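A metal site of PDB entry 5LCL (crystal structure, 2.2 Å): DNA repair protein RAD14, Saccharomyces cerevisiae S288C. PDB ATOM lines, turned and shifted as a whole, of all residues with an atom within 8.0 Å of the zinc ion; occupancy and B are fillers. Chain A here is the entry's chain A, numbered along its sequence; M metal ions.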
ATOM      1  N   LYS A   3     -20.201  25.010  17.269  1.00  0.00           N
ATOM      2  CA  LYS A   3     -20.124  23.867  16.359  1.00  0.00           C
ATOM      3  C   LYS A   3     -19.555  22.604  17.005  1.00  0.00           C
ATOM      4  O   LYS A   3     -18.749  22.669  17.918  1.00  0.00           O
ATOM      5  CB  LYS A   3     -19.263  24.220  15.116  1.00  0.00           C
ATOM      6  CG  LYS A   3     -19.680  25.526  14.428  1.00  0.00           C
ATOM      7  CD  LYS A   3     -20.892  25.282  13.552  1.00  0.00           C
ATOM      8  CE  LYS A   3     -21.480  26.562  13.002  1.00  0.00           C
ATOM      9  NZ  LYS A   3     -20.479  27.317  12.222  1.00  0.00           N
ATOM     10  N   CYS A   4     -19.975  21.452  16.516  1.00  0.00           N
ATOM     11  CA  CYS A   4     -19.358  20.209  16.868  1.00  0.00           C
ATOM     12  C   CYS A   4     -17.843  20.259  16.623  1.00  0.00           C
ATOM     13  O   CYS A   4     -17.362  20.661  15.581  1.00  0.00           O
ATOM     14  CB  CYS A   4     -19.935  19.091  16.026  1.00  0.00           C
ATOM     15  SG  CYS A   4     -19.098  17.532  16.200  1.00  0.00           S
ATOM     16  N   ILE A   5     -17.077  19.807  17.605  1.00  0.00           N
ATOM     17  CA  ILE A   5     -15.624  19.884  17.549  1.00  0.00           C
ATOM     18  C   ILE A   5     -14.996  18.889  16.541  1.00  0.00           C
ATOM     19  O   ILE A   5     -13.822  18.995  16.269  1.00  0.00           O
ATOM     20  CB  ILE A   5     -15.018  19.649  18.943  1.00  0.00           C
ATOM     21  CG1 ILE A   5     -15.268  18.169  19.351  1.00  0.00           C
ATOM     22  CG2 ILE A   5     -15.560  20.635  19.984  1.00  0.00           C
ATOM     23  CD1 ILE A   5     -15.199  17.880  20.852  1.00  0.00           C
ATOM     24  N   GLU A   6     -15.733  17.916  15.993  1.00  0.00           N
ATOM     25  CA  GLU A   6     -15.166  16.976  15.036  1.00  0.00           C
ATOM     26  C   GLU A   6     -15.434  17.453  13.646  1.00  0.00           C
ATOM     27  O   GLU A   6     -14.523  17.580  12.870  1.00  0.00           O
ATOM     28  CB  GLU A   6     -15.798  15.611  15.179  1.00  0.00           C
ATOM     29  CG  GLU A   6     -15.406  14.883  16.419  1.00  0.00           C
ATOM     30  CD  GLU A   6     -13.985  14.368  16.395  1.00  0.00           C
ATOM     31  OE1 GLU A   6     -13.468  14.033  17.437  1.00  0.00           O
ATOM     32  OE2 GLU A   6     -13.353  14.285  15.336  1.00  0.00           O
ATOM     33  N   CYS A   7     -16.709  17.733  13.331  1.00  0.00           N
ATOM     34  CA  CYS A   7     -17.067  18.191  11.977  1.00  0.00           C
ATOM     35  C   CYS A   7     -17.009  19.675  11.785  1.00  0.00           C
ATOM     36  O   CYS A   7     -16.892  20.158  10.618  1.00  0.00           O
ATOM     37  CB  CYS A   7     -18.431  17.667  11.501  1.00  0.00           C
ATOM     38  SG  CYS A   7     -19.905  18.156  12.419  1.00  0.00           S
ATOM     39  N   HIS A   8     -17.104  20.440  12.875  1.00  0.00           N
ATOM     40  CA  HIS A   8     -17.263  21.902  12.790  1.00  0.00           C
ATOM     41  C   HIS A   8     -18.426  22.321  11.902  1.00  0.00           C
ATOM     42  O   HIS A   8     -18.373  23.394  11.291  1.00  0.00           O
ATOM     43  CB  HIS A   8     -15.964  22.570  12.297  1.00  0.00           C
ATOM     44  CG  HIS A   8     -14.721  21.980  12.887  1.00  0.00           C
ATOM     45  ND1 HIS A   8     -14.398  22.114  14.218  1.00  0.00           N
ATOM     46  CD2 HIS A   8     -13.700  21.302  12.306  1.00  0.00           C
ATOM     47  CE1 HIS A   8     -13.237  21.517  14.448  1.00  0.00           C
ATOM     48  NE2 HIS A   8     -12.789  21.028  13.300  1.00  0.00           N
ATOM     49  N   ILE A   9     -19.481  21.527  11.836  1.00  0.00           N
ATOM     50  CA  ILE A   9     -20.614  21.891  11.015  1.00  0.00           C
ATOM     51  C   ILE A   9     -21.899  21.840  11.790  1.00  0.00           C
ATOM     52  O   ILE A   9     -22.595  22.863  11.915  1.00  0.00           O
ATOM     53  CB  ILE A   9     -20.660  21.002   9.743  1.00  0.00           C
ATOM     54  CG1 ILE A   9     -19.507  21.418   8.775  1.00  0.00           C
ATOM     55  CG2 ILE A   9     -22.004  21.140   9.029  1.00  0.00           C
ATOM     56  CD1 ILE A   9     -19.059  20.310   7.839  1.00  0.00           C
ATOM     57  N   ASN A  10     -22.206  20.664  12.352  1.00  0.00           N
ATOM     58  CA  ASN A  10     -23.423  20.521  13.171  1.00  0.00           C
ATOM     59  C   ASN A  10     -23.410  21.408  14.401  1.00  0.00           C
ATOM     60  O   ASN A  10     -22.367  21.688  14.973  1.00  0.00           O
ATOM     61  CB  ASN A  10     -23.727  19.089  13.590  1.00  0.00           C
ATOM     62  CG  ASN A  10     -24.458  18.347  12.526  1.00  0.00           C
ATOM     63  OD1 ASN A  10     -25.257  18.955  11.774  1.00  0.00           O
ATOM     64  ND2 ASN A  10     -24.242  17.022  12.460  1.00  0.00           N
ATOM     65  N   ILE A  11     -24.586  21.914  14.718  1.00  0.00           N
ATOM     66  CA  ILE A  11     -24.774  22.729  15.854  1.00  0.00           C
ATOM     67  C   ILE A  11     -25.663  22.042  16.908  1.00  0.00           C
ATOM     68  O   ILE A  11     -25.826  22.616  17.960  1.00  0.00           O
ATOM     69  CB  ILE A  11     -25.373  24.101  15.497  1.00  0.00           C
ATOM     70  CG1 ILE A  11     -26.712  23.980  14.757  1.00  0.00           C
ATOM     71  CG2 ILE A  11     -24.360  24.926  14.707  1.00  0.00           C
ATOM     72  CD1 ILE A  11     -27.501  25.274  14.757  1.00  0.00           C
ATOM     73  N   GLU A  12     -26.237  20.874  16.625  1.00  0.00           N
ATOM     74  CA  GLU A  12     -27.026  20.140  17.613  1.00  0.00           C
ATOM     75  C   GLU A  12     -26.193  19.029  18.110  1.00  0.00           C
ATOM     76  O   GLU A  12     -25.894  18.134  17.377  1.00  0.00           O
ATOM     77  CB  GLU A  12     -28.268  19.555  17.004  1.00  0.00           C
ATOM     78  CG  GLU A  12     -29.265  20.572  16.535  1.00  0.00           C
ATOM     79  CD  GLU A  12     -30.639  20.172  17.001  1.00  0.00           C
ATOM     80  OE1 GLU A  12     -30.800  19.936  18.248  1.00  0.00           O
ATOM     81  OE2 GLU A  12     -31.533  20.036  16.141  1.00  0.00           O
ATOM     82  N   MET A  13     -25.865  19.078  19.368  1.00  0.00           N
ATOM     83  CA  MET A  13     -24.975  18.157  19.989  1.00  0.00           C
ATOM     84  C   MET A  13     -25.744  16.942  20.466  1.00  0.00           C
ATOM     85  O   MET A  13     -26.943  16.961  20.645  1.00  0.00           O
ATOM     86  CB  MET A  13     -24.254  18.838  21.150  1.00  0.00           C
ATOM     87  CG  MET A  13     -23.567  20.131  20.796  1.00  0.00           C
ATOM     88  SD  MET A  13     -22.391  19.949  19.419  1.00  0.00           S
ATOM     89  CE  MET A  13     -22.446  21.606  18.771  1.00  0.00           C
ATOM     90  N   GLN A  24     -19.006  18.622  23.304  1.00  0.00           N
ATOM     91  CA  GLN A  24     -19.740  19.234  22.176  1.00  0.00           C
ATOM     92  C   GLN A  24     -19.471  18.430  20.901  1.00  0.00           C
ATOM     93  O   GLN A  24     -18.627  18.847  20.053  1.00  0.00           O
ATOM     94  CB  GLN A  24     -19.243  20.641  21.896  1.00  0.00           C
ATOM     95  CG  GLN A  24     -19.246  21.527  23.064  1.00  0.00           C
ATOM     96  CD  GLN A  24     -19.711  22.855  22.632  1.00  0.00           C
ATOM     97  OE1 GLN A  24     -19.105  23.504  21.762  1.00  0.00           O
ATOM     98  NE2 GLN A  24     -20.881  23.223  23.144  1.00  0.00           N
ATOM     99  N   VAL A  25     -20.153  17.293  20.788  1.00  0.00           N
ATOM    100  CA  VAL A  25     -20.012  16.409  19.633  1.00  0.00           C
ATOM    101  C   VAL A  25     -21.402  16.070  19.133  1.00  0.00           C
ATOM    102  O   VAL A  25     -22.289  15.805  19.952  1.00  0.00           O
ATOM    103  CB  VAL A  25     -19.315  15.097  20.013  1.00  0.00           C
ATOM    104  CG1 VAL A  25     -19.019  14.303  18.771  1.00  0.00           C
ATOM    105  CG2 VAL A  25     -18.005  15.371  20.705  1.00  0.00           C
ATOM    106  N   CYS A  26     -21.585  16.048  17.804  1.00  0.00           N
ATOM    107  CA  CYS A  26     -22.874  15.708  17.245  1.00  0.00           C
ATOM    108  C   CYS A  26     -22.997  14.189  17.276  1.00  0.00           C
ATOM    109  O   CYS A  26     -22.000  13.495  17.359  1.00  0.00           O
ATOM    110  CB  CYS A  26     -23.086  16.284  15.833  1.00  0.00           C
ATOM    111  SG  CYS A  26     -22.106  15.588  14.507  1.00  0.00           S
ATOM    112  N   LYS A  27     -24.224  13.707  17.237  1.00  0.00           N
ATOM    113  CA  LYS A  27     -24.517  12.289  17.209  1.00  0.00           C
ATOM    114  C   LYS A  27     -23.850  11.586  16.048  1.00  0.00           C
ATOM    115  O   LYS A  27     -23.239  10.521  16.250  1.00  0.00           O
ATOM    116  CB  LYS A  27     -26.022  12.078  17.184  1.00  0.00           C
ATOM    117  CG  LYS A  27     -26.408  10.609  17.167  1.00  0.00           C
ATOM    118  CD  LYS A  27     -27.701  10.259  17.920  1.00  0.00           C
ATOM    119  CE  LYS A  27     -28.051   8.770  17.695  1.00  0.00           C
ATOM    120  NZ  LYS A  27     -28.354   7.967  18.925  1.00  0.00           N
ATOM    121  N   GLN A  28     -23.926  12.149  14.849  1.00  0.00           N
ATOM    122  CA  GLN A  28     -23.283  11.534  13.675  1.00  0.00           C
ATOM    123  C   GLN A  28     -21.743  11.290  13.876  1.00  0.00           C
ATOM    124  O   GLN A  28     -21.220  10.201  13.596  1.00  0.00           O
ATOM    125  CB  GLN A  28     -23.561  12.343  12.414  1.00  0.00           C
ATOM    126  CG  GLN A  28     -22.822  11.817  11.178  1.00  0.00           C
ATOM    127  CD  GLN A  28     -23.291  12.469   9.899  1.00  0.00           C
ATOM    128  OE1 GLN A  28     -24.159  13.327   9.916  1.00  0.00           O
ATOM    129  NE2 GLN A  28     -22.680  12.096   8.792  1.00  0.00           N
ATOM    130  N   CYS A  29     -21.064  12.327  14.350  1.00  0.00           N
ATOM    131  CA  CYS A  29     -19.621  12.261  14.595  1.00  0.00           C
ATOM    132  C   CYS A  29     -19.278  11.223  15.668  1.00  0.00           C
ATOM    133  O   CYS A  29     -18.233  10.548  15.588  1.00  0.00           O
ATOM    134  CB  CYS A  29     -19.066  13.657  14.914  1.00  0.00           C
ATOM    135  SG  CYS A  29     -18.942  14.727  13.476  1.00  0.00           S
ATOM    136  N   SER A  30     -20.182  11.063  16.633  1.00  0.00           N
ATOM    137  CA  SER A  30     -19.989  10.053  17.656  1.00  0.00           C
ATOM    138  C   SER A  30     -20.020   8.634  17.103  1.00  0.00           C
ATOM    139  O   SER A  30     -19.254   7.806  17.602  1.00  0.00           O
ATOM    140  CB  SER A  30     -20.974  10.215  18.805  1.00  0.00           C
ATOM    141  OG  SER A  30     -22.150   9.501  18.635  1.00  0.00           O
ATOM    142  N   GLU A  32     -19.321   7.946  13.895  1.00  0.00           N
ATOM    143  CA  GLU A  32     -18.162   7.952  13.016  1.00  0.00           C
ATOM    144  C   GLU A  32     -16.843   7.730  13.776  1.00  0.00           C
ATOM    145  O   GLU A  32     -15.877   7.303  13.153  1.00  0.00           O
ATOM    146  CB  GLU A  32     -18.107   9.256  12.203  1.00  0.00           C
ATOM    147  CG  GLU A  32     -19.087   9.247  11.025  1.00  0.00           C
ATOM    148  CD  GLU A  32     -19.444  10.576  10.382  1.00  0.00           C
ATOM    149  OE1 GLU A  32     -19.053  11.665  10.825  1.00  0.00           O
ATOM    150  OE2 GLU A  32     -20.200  10.480   9.404  1.00  0.00           O
ATOM    151  N   HIS A  33     -16.794   8.038  15.078  1.00  0.00           N
ATOM    152  CA  HIS A  33     -15.543   7.924  15.806  1.00  0.00           C
ATOM    153  C   HIS A  33     -15.749   7.195  17.123  1.00  0.00           C
ATOM    154  O   HIS A  33     -15.589   7.786  18.193  1.00  0.00           O
ATOM    155  CB  HIS A  33     -14.987   9.326  16.051  1.00  0.00           C
ATOM    156  CG  HIS A  33     -14.597  10.039  14.796  1.00  0.00           C
ATOM    157  ND1 HIS A  33     -13.579   9.589  13.983  1.00  0.00           N
ATOM    158  CD2 HIS A  33     -15.096  11.143  14.199  1.00  0.00           C
ATOM    159  CE1 HIS A  33     -13.463  10.393  12.942  1.00  0.00           C
ATOM    160  NE2 HIS A  33     -14.349  11.350  13.062  1.00  0.00           N
ATOM    161  N   TYR A  37     -15.679   8.116  21.162  1.00  0.00           N
ATOM    162  CA  TYR A  37     -16.989   8.424  21.736  1.00  0.00           C
ATOM    163  C   TYR A  37     -17.848   7.227  22.118  1.00  0.00           C
ATOM    164  O   TYR A  37     -18.919   7.444  22.698  1.00  0.00           O
ATOM    165  CB  TYR A  37     -17.762   9.362  20.799  1.00  0.00           C
ATOM    166  CG  TYR A  37     -16.923  10.561  20.449  1.00  0.00           C
ATOM    167  CD1 TYR A  37     -16.526  11.439  21.429  1.00  0.00           C
ATOM    168  CD2 TYR A  37     -16.480  10.785  19.181  1.00  0.00           C
ATOM    169  CE1 TYR A  37     -15.737  12.527  21.147  1.00  0.00           C
ATOM    170  CE2 TYR A  37     -15.683  11.884  18.884  1.00  0.00           C
ATOM    171  CZ  TYR A  37     -15.311  12.743  19.892  1.00  0.00           C
ATOM    172  OH  TYR A  37     -14.517  13.867  19.678  1.00  0.00           O
HETATM  173 ZN    ZN M   1     -20.052  16.609  14.200  1.00  0.00          ZN
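SG of Cys 26 sits close to ND2 of Asn 10. The backbone NH (N) of Asn 10 lies close to the side-chain sulfur (SG) of Cys 7. The side-chain sulfur (SG) of Cys 7 sits close to the backbone NH (N) of Ile 9 (3.4 Å). The backbone carbonyl oxygen (O) of Asn 10 lies within hydrogen-bond range of the backbone NH (N) of Cys 4 (2.9 Å). The backbone NH (N) of Glu 6 sits close to the side-chain sulfur (SG) of Cys 4 (3.4 Å).
Four residues have an atom within 4 Å of the zinc ion: Cys 4, Cys 7, Cys 26 and Cys 29.
The zinc ion is bound by the side-chain sulfur of Cys 29 (2.3 Å), the side-chain sulfur of Cys 26 (2.3 Å), the side-chain sulfur of Cys 7 (2.4 Å) and the side-chain sulfur of Cys 4 (2.4 Å).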
